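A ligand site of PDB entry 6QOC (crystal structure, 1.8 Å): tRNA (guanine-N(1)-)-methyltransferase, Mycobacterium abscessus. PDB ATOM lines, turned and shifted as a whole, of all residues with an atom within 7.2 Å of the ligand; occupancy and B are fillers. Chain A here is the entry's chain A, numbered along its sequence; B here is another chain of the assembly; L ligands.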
ATOM      1  N   VAL A  84       4.770   6.653 -13.549  1.00  0.00           N
ATOM      2  CA  VAL A  84       4.047   5.942 -14.607  1.00  0.00           C
ATOM      3  C   VAL A  84       4.965   4.911 -15.282  1.00  0.00           C
ATOM      4  O   VAL A  84       5.816   5.282 -16.097  1.00  0.00           O
ATOM      5  CB  VAL A  84       3.504   6.896 -15.701  1.00  0.00           C
ATOM      6  CG1 VAL A  84       2.640   6.124 -16.695  1.00  0.00           C
ATOM      7  CG2 VAL A  84       2.722   8.050 -15.084  1.00  0.00           C
ATOM      8  N   PRO A  85       4.831   3.630 -14.916  1.00  0.00           N
ATOM      9  CA  PRO A  85       5.652   2.624 -15.595  1.00  0.00           C
ATOM     10  C   PRO A  85       5.252   2.498 -17.064  1.00  0.00           C
ATOM     11  O   PRO A  85       4.063   2.340 -17.392  1.00  0.00           O
ATOM     12  CB  PRO A  85       5.381   1.341 -14.799  1.00  0.00           C
ATOM     13  CG  PRO A  85       4.901   1.839 -13.417  1.00  0.00           C
ATOM     14  CD  PRO A  85       4.112   3.086 -13.744  1.00  0.00           C
ATOM     15  N   THR A  86       6.238   2.571 -17.944  1.00  0.00           N
ATOM     16  CA  THR A  86       5.997   2.503 -19.379  1.00  0.00           C
ATOM     17  C   THR A  86       7.255   2.011 -20.093  1.00  0.00           C
ATOM     18  O   THR A  86       8.377   2.297 -19.648  1.00  0.00           O
ATOM     19  CB  THR A  86       5.554   3.891 -19.945  1.00  0.00           C
ATOM     20  OG1 THR A  86       5.632   3.873 -21.381  1.00  0.00           O
ATOM     21  CG2 THR A  86       6.417   4.997 -19.413  1.00  0.00           C
ATOM     22  N   PRO A  87       7.065   1.236 -21.167  1.00  0.00           N
ATOM     23  CA  PRO A  87       8.192   0.755 -21.972  1.00  0.00           C
ATOM     24  C   PRO A  87       8.979   1.911 -22.576  1.00  0.00           C
ATOM     25  O   PRO A  87      10.156   1.768 -22.897  1.00  0.00           O
ATOM     26  CB  PRO A  87       7.507  -0.066 -23.073  1.00  0.00           C
ATOM     27  CG  PRO A  87       6.139   0.560 -23.205  1.00  0.00           C
ATOM     28  CD  PRO A  87       5.765   0.877 -21.778  1.00  0.00           C
ATOM     29  N   ALA A  88       8.320   3.053 -22.722  1.00  0.00           N
ATOM     30  CA  ALA A  88       8.929   4.229 -23.321  1.00  0.00           C
ATOM     31  C   ALA A  88       9.492   5.192 -22.262  1.00  0.00           C
ATOM     32  O   ALA A  88       9.761   6.352 -22.549  1.00  0.00           O
ATOM     33  CB  ALA A  88       7.892   4.942 -24.196  1.00  0.00           C
ATOM     34  N   GLY A  89       9.662   4.702 -21.035  1.00  0.00           N
ATOM     35  CA  GLY A  89      10.098   5.544 -19.931  1.00  0.00           C
ATOM     36  C   GLY A  89      11.598   5.764 -19.867  1.00  0.00           C
ATOM     37  O   GLY A  89      12.367   5.087 -20.565  1.00  0.00           O
ATOM     38  N   ALA A 109       0.715   4.908 -11.394  1.00  0.00           N
ATOM     39  CA  ALA A 109      -0.354   4.693 -12.344  1.00  0.00           C
ATOM     40  C   ALA A 109      -0.053   3.522 -13.275  1.00  0.00           C
ATOM     41  O   ALA A 109       0.794   3.628 -14.179  1.00  0.00           O
ATOM     42  CB  ALA A 109      -0.596   5.975 -13.147  1.00  0.00           C
ATOM     43  N   CYS A 110      -0.741   2.402 -13.067  1.00  0.00           N
ATOM     44  CA  CYS A 110      -0.505   1.198 -13.846  1.00  0.00           C
ATOM     45  C   CYS A 110      -1.386   1.149 -15.068  1.00  0.00           C
ATOM     46  O   CYS A 110      -2.594   1.056 -14.951  1.00  0.00           O
ATOM     47  CB  CYS A 110      -0.749  -0.064 -13.013  1.00  0.00           C
ATOM     48  SG  CYS A 110       0.297  -0.156 -11.575  1.00  0.00           S
ATOM     49  N   GLY A 111      -0.787   1.197 -16.254  1.00  0.00           N
ATOM     50  CA  GLY A 111      -1.554   1.116 -17.479  1.00  0.00           C
ATOM     51  C   GLY A 111      -1.177  -0.089 -18.314  1.00  0.00           C
ATOM     52  O   GLY A 111      -0.192  -0.778 -18.051  1.00  0.00           O
ATOM     53  N   ARG A 112      -1.980  -0.358 -19.330  1.00  0.00           N
ATOM     54  CA  ARG A 112      -1.641  -1.394 -20.309  1.00  0.00           C
ATOM     55  C   ARG A 112      -0.458  -0.974 -21.199  1.00  0.00           C
ATOM     56  O   ARG A 112      -0.120   0.215 -21.281  1.00  0.00           O
ATOM     57  CB  ARG A 112      -2.850  -1.699 -21.166  1.00  0.00           C
ATOM     58  CG  ARG A 112      -3.365  -0.474 -21.889  1.00  0.00           C
ATOM     59  CD  ARG A 112      -4.637  -0.814 -22.640  1.00  0.00           C
ATOM     60  NE  ARG A 112      -4.403  -1.912 -23.582  1.00  0.00           N
ATOM     61  CZ  ARG A 112      -5.282  -2.858 -23.861  1.00  0.00           C
ATOM     62  NH1 ARG A 112      -4.978  -3.812 -24.739  1.00  0.00           N
ATOM     63  NH2 ARG A 112      -6.475  -2.854 -23.281  1.00  0.00           N
ATOM     64  N   TYR A 113       0.140  -1.955 -21.869  1.00  0.00           N
ATOM     65  CA  TYR A 113       1.310  -1.742 -22.715  1.00  0.00           C
ATOM     66  C   TYR A 113       1.077  -0.647 -23.758  1.00  0.00           C
ATOM     67  O   TYR A 113       1.948   0.194 -24.024  1.00  0.00           O
ATOM     68  CB  TYR A 113       1.701  -3.053 -23.415  1.00  0.00           C
ATOM     69  CG  TYR A 113       2.770  -2.910 -24.466  1.00  0.00           C
ATOM     70  CD1 TYR A 113       3.973  -2.253 -24.181  1.00  0.00           C
ATOM     71  CD2 TYR A 113       2.599  -3.435 -25.742  1.00  0.00           C
ATOM     72  CE1 TYR A 113       4.971  -2.121 -25.143  1.00  0.00           C
ATOM     73  CE2 TYR A 113       3.586  -3.315 -26.717  1.00  0.00           C
ATOM     74  CZ  TYR A 113       4.769  -2.655 -26.400  1.00  0.00           C
ATOM     75  OH  TYR A 113       5.758  -2.519 -27.358  1.00  0.00           O
ATOM     76  N   GLU A 114      -0.122  -0.670 -24.320  1.00  0.00           N
ATOM     77  CA  GLU A 114      -0.526   0.251 -25.389  1.00  0.00           C
ATOM     78  C   GLU A 114      -0.483   1.717 -24.955  1.00  0.00           C
ATOM     79  O   GLU A 114      -0.266   2.606 -25.772  1.00  0.00           O
ATOM     80  CB  GLU A 114      -1.921  -0.115 -25.863  1.00  0.00           C
ATOM     81  CG  GLU A 114      -2.037  -1.491 -26.466  1.00  0.00           C
ATOM     82  CD  GLU A 114      -1.136  -1.669 -27.653  1.00  0.00           C
ATOM     83  OE1 GLU A 114      -1.021  -0.705 -28.452  1.00  0.00           O
ATOM     84  OE2 GLU A 114      -0.533  -2.752 -27.793  1.00  0.00           O
ATOM     85  N   GLY A 115      -0.734   1.951 -23.671  1.00  0.00           N
ATOM     86  CA  GLY A 115      -0.512   3.245 -23.066  1.00  0.00           C
ATOM     87  C   GLY A 115      -1.728   3.949 -22.492  1.00  0.00           C
ATOM     88  O   GLY A 115      -2.875   3.606 -22.780  1.00  0.00           O
ATOM     89  N   VAL A 133       8.739   5.845 -16.393  1.00  0.00           N
ATOM     90  CA  VAL A 133       9.948   5.043 -16.202  1.00  0.00           C
ATOM     91  C   VAL A 133       9.783   3.610 -16.675  1.00  0.00           C
ATOM     92  O   VAL A 133       8.690   3.045 -16.573  1.00  0.00           O
ATOM     93  CB  VAL A 133      10.391   5.014 -14.720  1.00  0.00           C
ATOM     94  CG1 VAL A 133      10.859   6.398 -14.236  1.00  0.00           C
ATOM     95  CG2 VAL A 133       9.282   4.473 -13.812  1.00  0.00           C
ATOM     96  N   SER A 134      10.877   3.052 -17.216  1.00  0.00           N
ATOM     97  CA  SER A 134      10.923   1.644 -17.588  1.00  0.00           C
ATOM     98  C   SER A 134      11.842   0.887 -16.616  1.00  0.00           C
ATOM     99  O   SER A 134      12.873   1.409 -16.185  1.00  0.00           O
ATOM    100  CB  SER A 134      11.422   1.481 -19.025  1.00  0.00           C
ATOM    101  OG  SER A 134      12.785   1.858 -19.104  1.00  0.00           O
ATOM    102  N   ILE A 135      11.470  -0.341 -16.256  1.00  0.00           N
ATOM    103  CA  ILE A 135      12.332  -1.118 -15.363  1.00  0.00           C
ATOM    104  C   ILE A 135      13.285  -2.045 -16.116  1.00  0.00           C
ATOM    105  O   ILE A 135      14.079  -2.757 -15.518  1.00  0.00           O
ATOM    106  CB  ILE A 135      11.512  -1.959 -14.358  1.00  0.00           C
ATOM    107  CG1 ILE A 135      10.569  -2.928 -15.097  1.00  0.00           C
ATOM    108  CG2 ILE A 135      10.752  -1.062 -13.387  1.00  0.00           C
ATOM    109  CD1 ILE A 135      10.083  -4.076 -14.176  1.00  0.00           C
ATOM    110  N   GLY A 136      13.219  -2.034 -17.452  1.00  0.00           N
ATOM    111  CA  GLY A 136      14.075  -2.885 -18.258  1.00  0.00           C
ATOM    112  C   GLY A 136      13.629  -2.976 -19.706  1.00  0.00           C
ATOM    113  O   GLY A 136      12.546  -2.497 -20.060  1.00  0.00           O
ATOM    114  N   ASP A 137      14.459  -3.604 -20.553  1.00  0.00           N
ATOM    115  CA  ASP A 137      14.155  -3.698 -21.973  1.00  0.00           C
ATOM    116  C   ASP A 137      13.533  -5.040 -22.315  1.00  0.00           C
ATOM    117  O   ASP A 137      14.131  -5.866 -22.983  1.00  0.00           O
ATOM    118  CB  ASP A 137      15.415  -3.477 -22.809  1.00  0.00           C
ATOM    119  CG  ASP A 137      16.003  -2.099 -22.604  1.00  0.00           C
ATOM    120  OD1 ASP A 137      15.243  -1.106 -22.748  1.00  0.00           O
ATOM    121  OD2 ASP A 137      17.199  -2.013 -22.294  1.00  0.00           O
ATOM    122  N   TYR A 138      12.344  -5.233 -21.796  1.00  0.00           N
ATOM    123  CA  TYR A 138      11.495  -6.354 -22.098  1.00  0.00           C
ATOM    124  C   TYR A 138      10.112  -5.741 -22.041  1.00  0.00           C
ATOM    125  O   TYR A 138       9.939  -4.687 -21.418  1.00  0.00           O
ATOM    126  CB  TYR A 138      11.665  -7.510 -21.105  1.00  0.00           C
ATOM    127  CG  TYR A 138      11.958  -7.021 -19.706  1.00  0.00           C
ATOM    128  CD1 TYR A 138      10.950  -6.520 -18.893  1.00  0.00           C
ATOM    129  CD2 TYR A 138      13.267  -7.033 -19.208  1.00  0.00           C
ATOM    130  CE1 TYR A 138      11.229  -6.048 -17.613  1.00  0.00           C
ATOM    131  CE2 TYR A 138      13.547  -6.568 -17.921  1.00  0.00           C
ATOM    132  CZ  TYR A 138      12.531  -6.081 -17.137  1.00  0.00           C
ATOM    133  OH  TYR A 138      12.819  -5.612 -15.860  1.00  0.00           O
ATOM    134  N   VAL A 139       9.156  -6.384 -22.684  1.00  0.00           N
ATOM    135  CA  VAL A 139       7.802  -5.875 -22.749  1.00  0.00           C
ATOM    136  C   VAL A 139       6.913  -6.643 -21.786  1.00  0.00           C
ATOM    137  O   VAL A 139       6.860  -7.867 -21.822  1.00  0.00           O
ATOM    138  CB  VAL A 139       7.221  -6.000 -24.176  1.00  0.00           C
ATOM    139  CG1 VAL A 139       5.791  -5.457 -24.207  1.00  0.00           C
ATOM    140  CG2 VAL A 139       8.092  -5.257 -25.181  1.00  0.00           C
ATOM    141  N   LEU A 140       6.185  -5.913 -20.945  1.00  0.00           N
ATOM    142  CA  LEU A 140       5.171  -6.505 -20.088  1.00  0.00           C
ATOM    143  C   LEU A 140       3.813  -6.139 -20.651  1.00  0.00           C
ATOM    144  O   LEU A 140       3.708  -5.164 -21.398  1.00  0.00           O
ATOM    145  CB  LEU A 140       5.288  -5.994 -18.654  1.00  0.00           C
ATOM    146  CG  LEU A 140       6.684  -6.043 -18.034  1.00  0.00           C
ATOM    147  CD1 LEU A 140       6.671  -5.329 -16.694  1.00  0.00           C
ATOM    148  CD2 LEU A 140       7.103  -7.498 -17.872  1.00  0.00           C
ATOM    149  N   ASN A 141       2.779  -6.867 -20.283  1.00  0.00           N
ATOM    150  CA  ASN A 141       1.450  -6.524 -20.783  1.00  0.00           C
ATOM    151  C   ASN A 141       0.858  -5.285 -20.118  1.00  0.00           C
ATOM    152  O   ASN A 141      -0.028  -4.632 -20.678  1.00  0.00           O
ATOM    153  CB  ASN A 141       0.488  -7.684 -20.592  1.00  0.00           C
ATOM    154  CG  ASN A 141      -0.164  -8.071 -21.889  1.00  0.00           C
ATOM    155  OD1 ASN A 141       0.522  -8.286 -22.886  1.00  0.00           O
ATOM    156  ND2 ASN A 141      -1.489  -8.115 -21.896  1.00  0.00           N
ATOM    157  N   GLY A 142       1.327  -4.973 -18.916  1.00  0.00           N
ATOM    158  CA  GLY A 142       0.850  -3.801 -18.189  1.00  0.00           C
ATOM    159  C   GLY A 142       1.834  -3.398 -17.116  1.00  0.00           C
ATOM    160  O   GLY A 142       2.797  -4.117 -16.870  1.00  0.00           O
ATOM    161  N   GLY A 143       1.606  -2.258 -16.463  1.00  0.00           N
ATOM    162  CA  GLY A 143       2.570  -1.737 -15.499  1.00  0.00           C
ATOM    163  C   GLY A 143       2.590  -2.378 -14.114  1.00  0.00           C
ATOM    164  O   GLY A 143       3.448  -2.045 -13.304  1.00  0.00           O
ATOM    165  N   GLU A 144       1.651  -3.298 -13.844  1.00  0.00           N
ATOM    166  CA  GLU A 144       1.517  -3.869 -12.504  1.00  0.00           C
ATOM    167  C   GLU A 144       2.800  -4.528 -11.974  1.00  0.00           C
ATOM    168  O   GLU A 144       3.229  -4.258 -10.846  1.00  0.00           O
ATOM    169  CB  GLU A 144       0.365  -4.875 -12.488  1.00  0.00           C
ATOM    170  CG  GLU A 144      -1.032  -4.239 -12.407  1.00  0.00           C
ATOM    171  CD  GLU A 144      -1.508  -3.658 -13.745  1.00  0.00           C
ATOM    172  OE1 GLU A 144      -0.892  -3.978 -14.794  1.00  0.00           O
ATOM    173  OE2 GLU A 144      -2.491  -2.886 -13.747  1.00  0.00           O
ATOM    174  N   ALA A 146       5.826  -4.011 -12.968  1.00  0.00           N
ATOM    175  CA  ALA A 146       6.828  -2.947 -12.795  1.00  0.00           C
ATOM    176  C   ALA A 146       6.575  -2.151 -11.518  1.00  0.00           C
ATOM    177  O   ALA A 146       7.530  -1.735 -10.837  1.00  0.00           O
ATOM    178  CB  ALA A 146       6.827  -2.035 -14.012  1.00  0.00           C
ATOM    179  N   VAL B 149       8.071 -10.685 -13.087  1.00  0.00           N
ATOM    180  CA  VAL B 149       8.428  -9.947 -14.307  1.00  0.00           C
ATOM    181  C   VAL B 149       8.774 -10.917 -15.418  1.00  0.00           C
ATOM    182  O   VAL B 149       8.261 -10.829 -16.535  1.00  0.00           O
ATOM    183  CB  VAL B 149       9.604  -8.980 -14.046  1.00  0.00           C
ATOM    184  CG1 VAL B 149      10.199  -8.470 -15.356  1.00  0.00           C
ATOM    185  CG2 VAL B 149       9.151  -7.831 -13.140  1.00  0.00           C
ATOM    186  N   ARG B 156       3.524 -13.731 -22.432  1.00  0.00           N
ATOM    187  CA  ARG B 156       2.798 -12.988 -23.461  1.00  0.00           C
ATOM    188  C   ARG B 156       3.347 -13.285 -24.864  1.00  0.00           C
ATOM    189  O   ARG B 156       2.740 -12.883 -25.870  1.00  0.00           O
ATOM    190  CB  ARG B 156       2.845 -11.486 -23.161  1.00  0.00           C
ATOM    191  CG  ARG B 156       4.198 -10.868 -23.263  1.00  0.00           C
ATOM    192  CD  ARG B 156       4.127  -9.396 -22.881  1.00  0.00           C
ATOM    193  NE  ARG B 156       3.378  -8.634 -23.875  1.00  0.00           N
ATOM    194  CZ  ARG B 156       3.862  -8.269 -25.050  1.00  0.00           C
ATOM    195  NH1 ARG B 156       5.108  -8.596 -25.403  1.00  0.00           N
ATOM    196  NH2 ARG B 156       3.105  -7.571 -25.894  1.00  0.00           N
HETATM  197  C1  LIG L   1       3.808  -0.737 -18.646  1.00  0.00           C
HETATM  198  N1  LIG L   1       6.286  -3.042 -21.138  1.00  0.00           N
HETATM  199  O1  LIG L   1       8.265  -2.566 -19.454  1.00  0.00           O
HETATM  200  C2  LIG L   1       9.482  -2.335 -18.877  1.00  0.00           C
HETATM  201  N2  LIG L   1       9.344  -1.364 -17.964  1.00  0.00           N
HETATM  202  C3  LIG L   1       8.050  -0.966 -17.943  1.00  0.00           C
HETATM  203  C4  LIG L   1       7.362  -1.717 -18.882  1.00  0.00           C
HETATM  204  C5  LIG L   1       5.998  -1.615 -19.172  1.00  0.00           C
HETATM  205  C6  LIG L   1       5.455  -2.267 -20.282  1.00  0.00           C
HETATM  206  C7  LIG L   1       4.101  -2.147 -20.566  1.00  0.00           C
HETATM  207  C8  LIG L   1       3.279  -1.394 -19.746  1.00  0.00           C
HETATM  208  C9  LIG L   1       5.162  -0.857 -18.362  1.00  0.00           C
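N of Ile 135 lies within hydrogen-bond range of N2 of the ligand, 2.9 Å away.
O of Leu 140 lies close to N1 of the ligand (3.3 Å).
The side-chain hydroxyl of Tyr 138 lies within hydrogen-bond range of the backbone carbonyl oxygen of Ile 135, at 3.1 Å.
N of Gly 143 is in hydrogen-bond range of O of Gly 111 (2.8 Å).
N of Thr 86 sits at hydrogen-bond distance from O of Val 133 (2.8 Å).
N of Ala 88 sits close to OG1 of Thr 86, 3.1 Å away.
The backbone NH (N) of Tyr 113 is in hydrogen-bond range of the backbone carbonyl oxygen (O) of Asn 141.
The backbone carbonyl oxygen (O) of Tyr 138 sits close to an oxygen (O1) of the ligand (3.3 Å).
Pro 85 touches the ligand (O to C1, 3.3 Å).
Thr 86 touches the ligand (CA to C9, 3.6 Å).
Pro 87 touches the ligand.
O of Gly 111 touches C8 of the ligand, 3.9 Å away.
CA of Tyr 113 touches C7 of the ligand, at 3.5 Å.
Ser 134 touches the ligand (CA to N2, 3.4 Å).
Gly 136 touches the ligand (O to C2, 3.3 Å).
CA of Val 139 touches N1 of the ligand, at 3.6 Å.
C of Gly 142 touches C8 of the ligand, 3.6 Å away.
N of Gly 143 touches C1 of the ligand, at 3.5 Å.
Hydrophobic or aromatic side chains within 4 Å of the ligand: Pro 87, Tyr 113, Ile 135, Val 139 and Leu 140.
Of the 28 residues printed, 13 come within 4 Å of the ligand.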
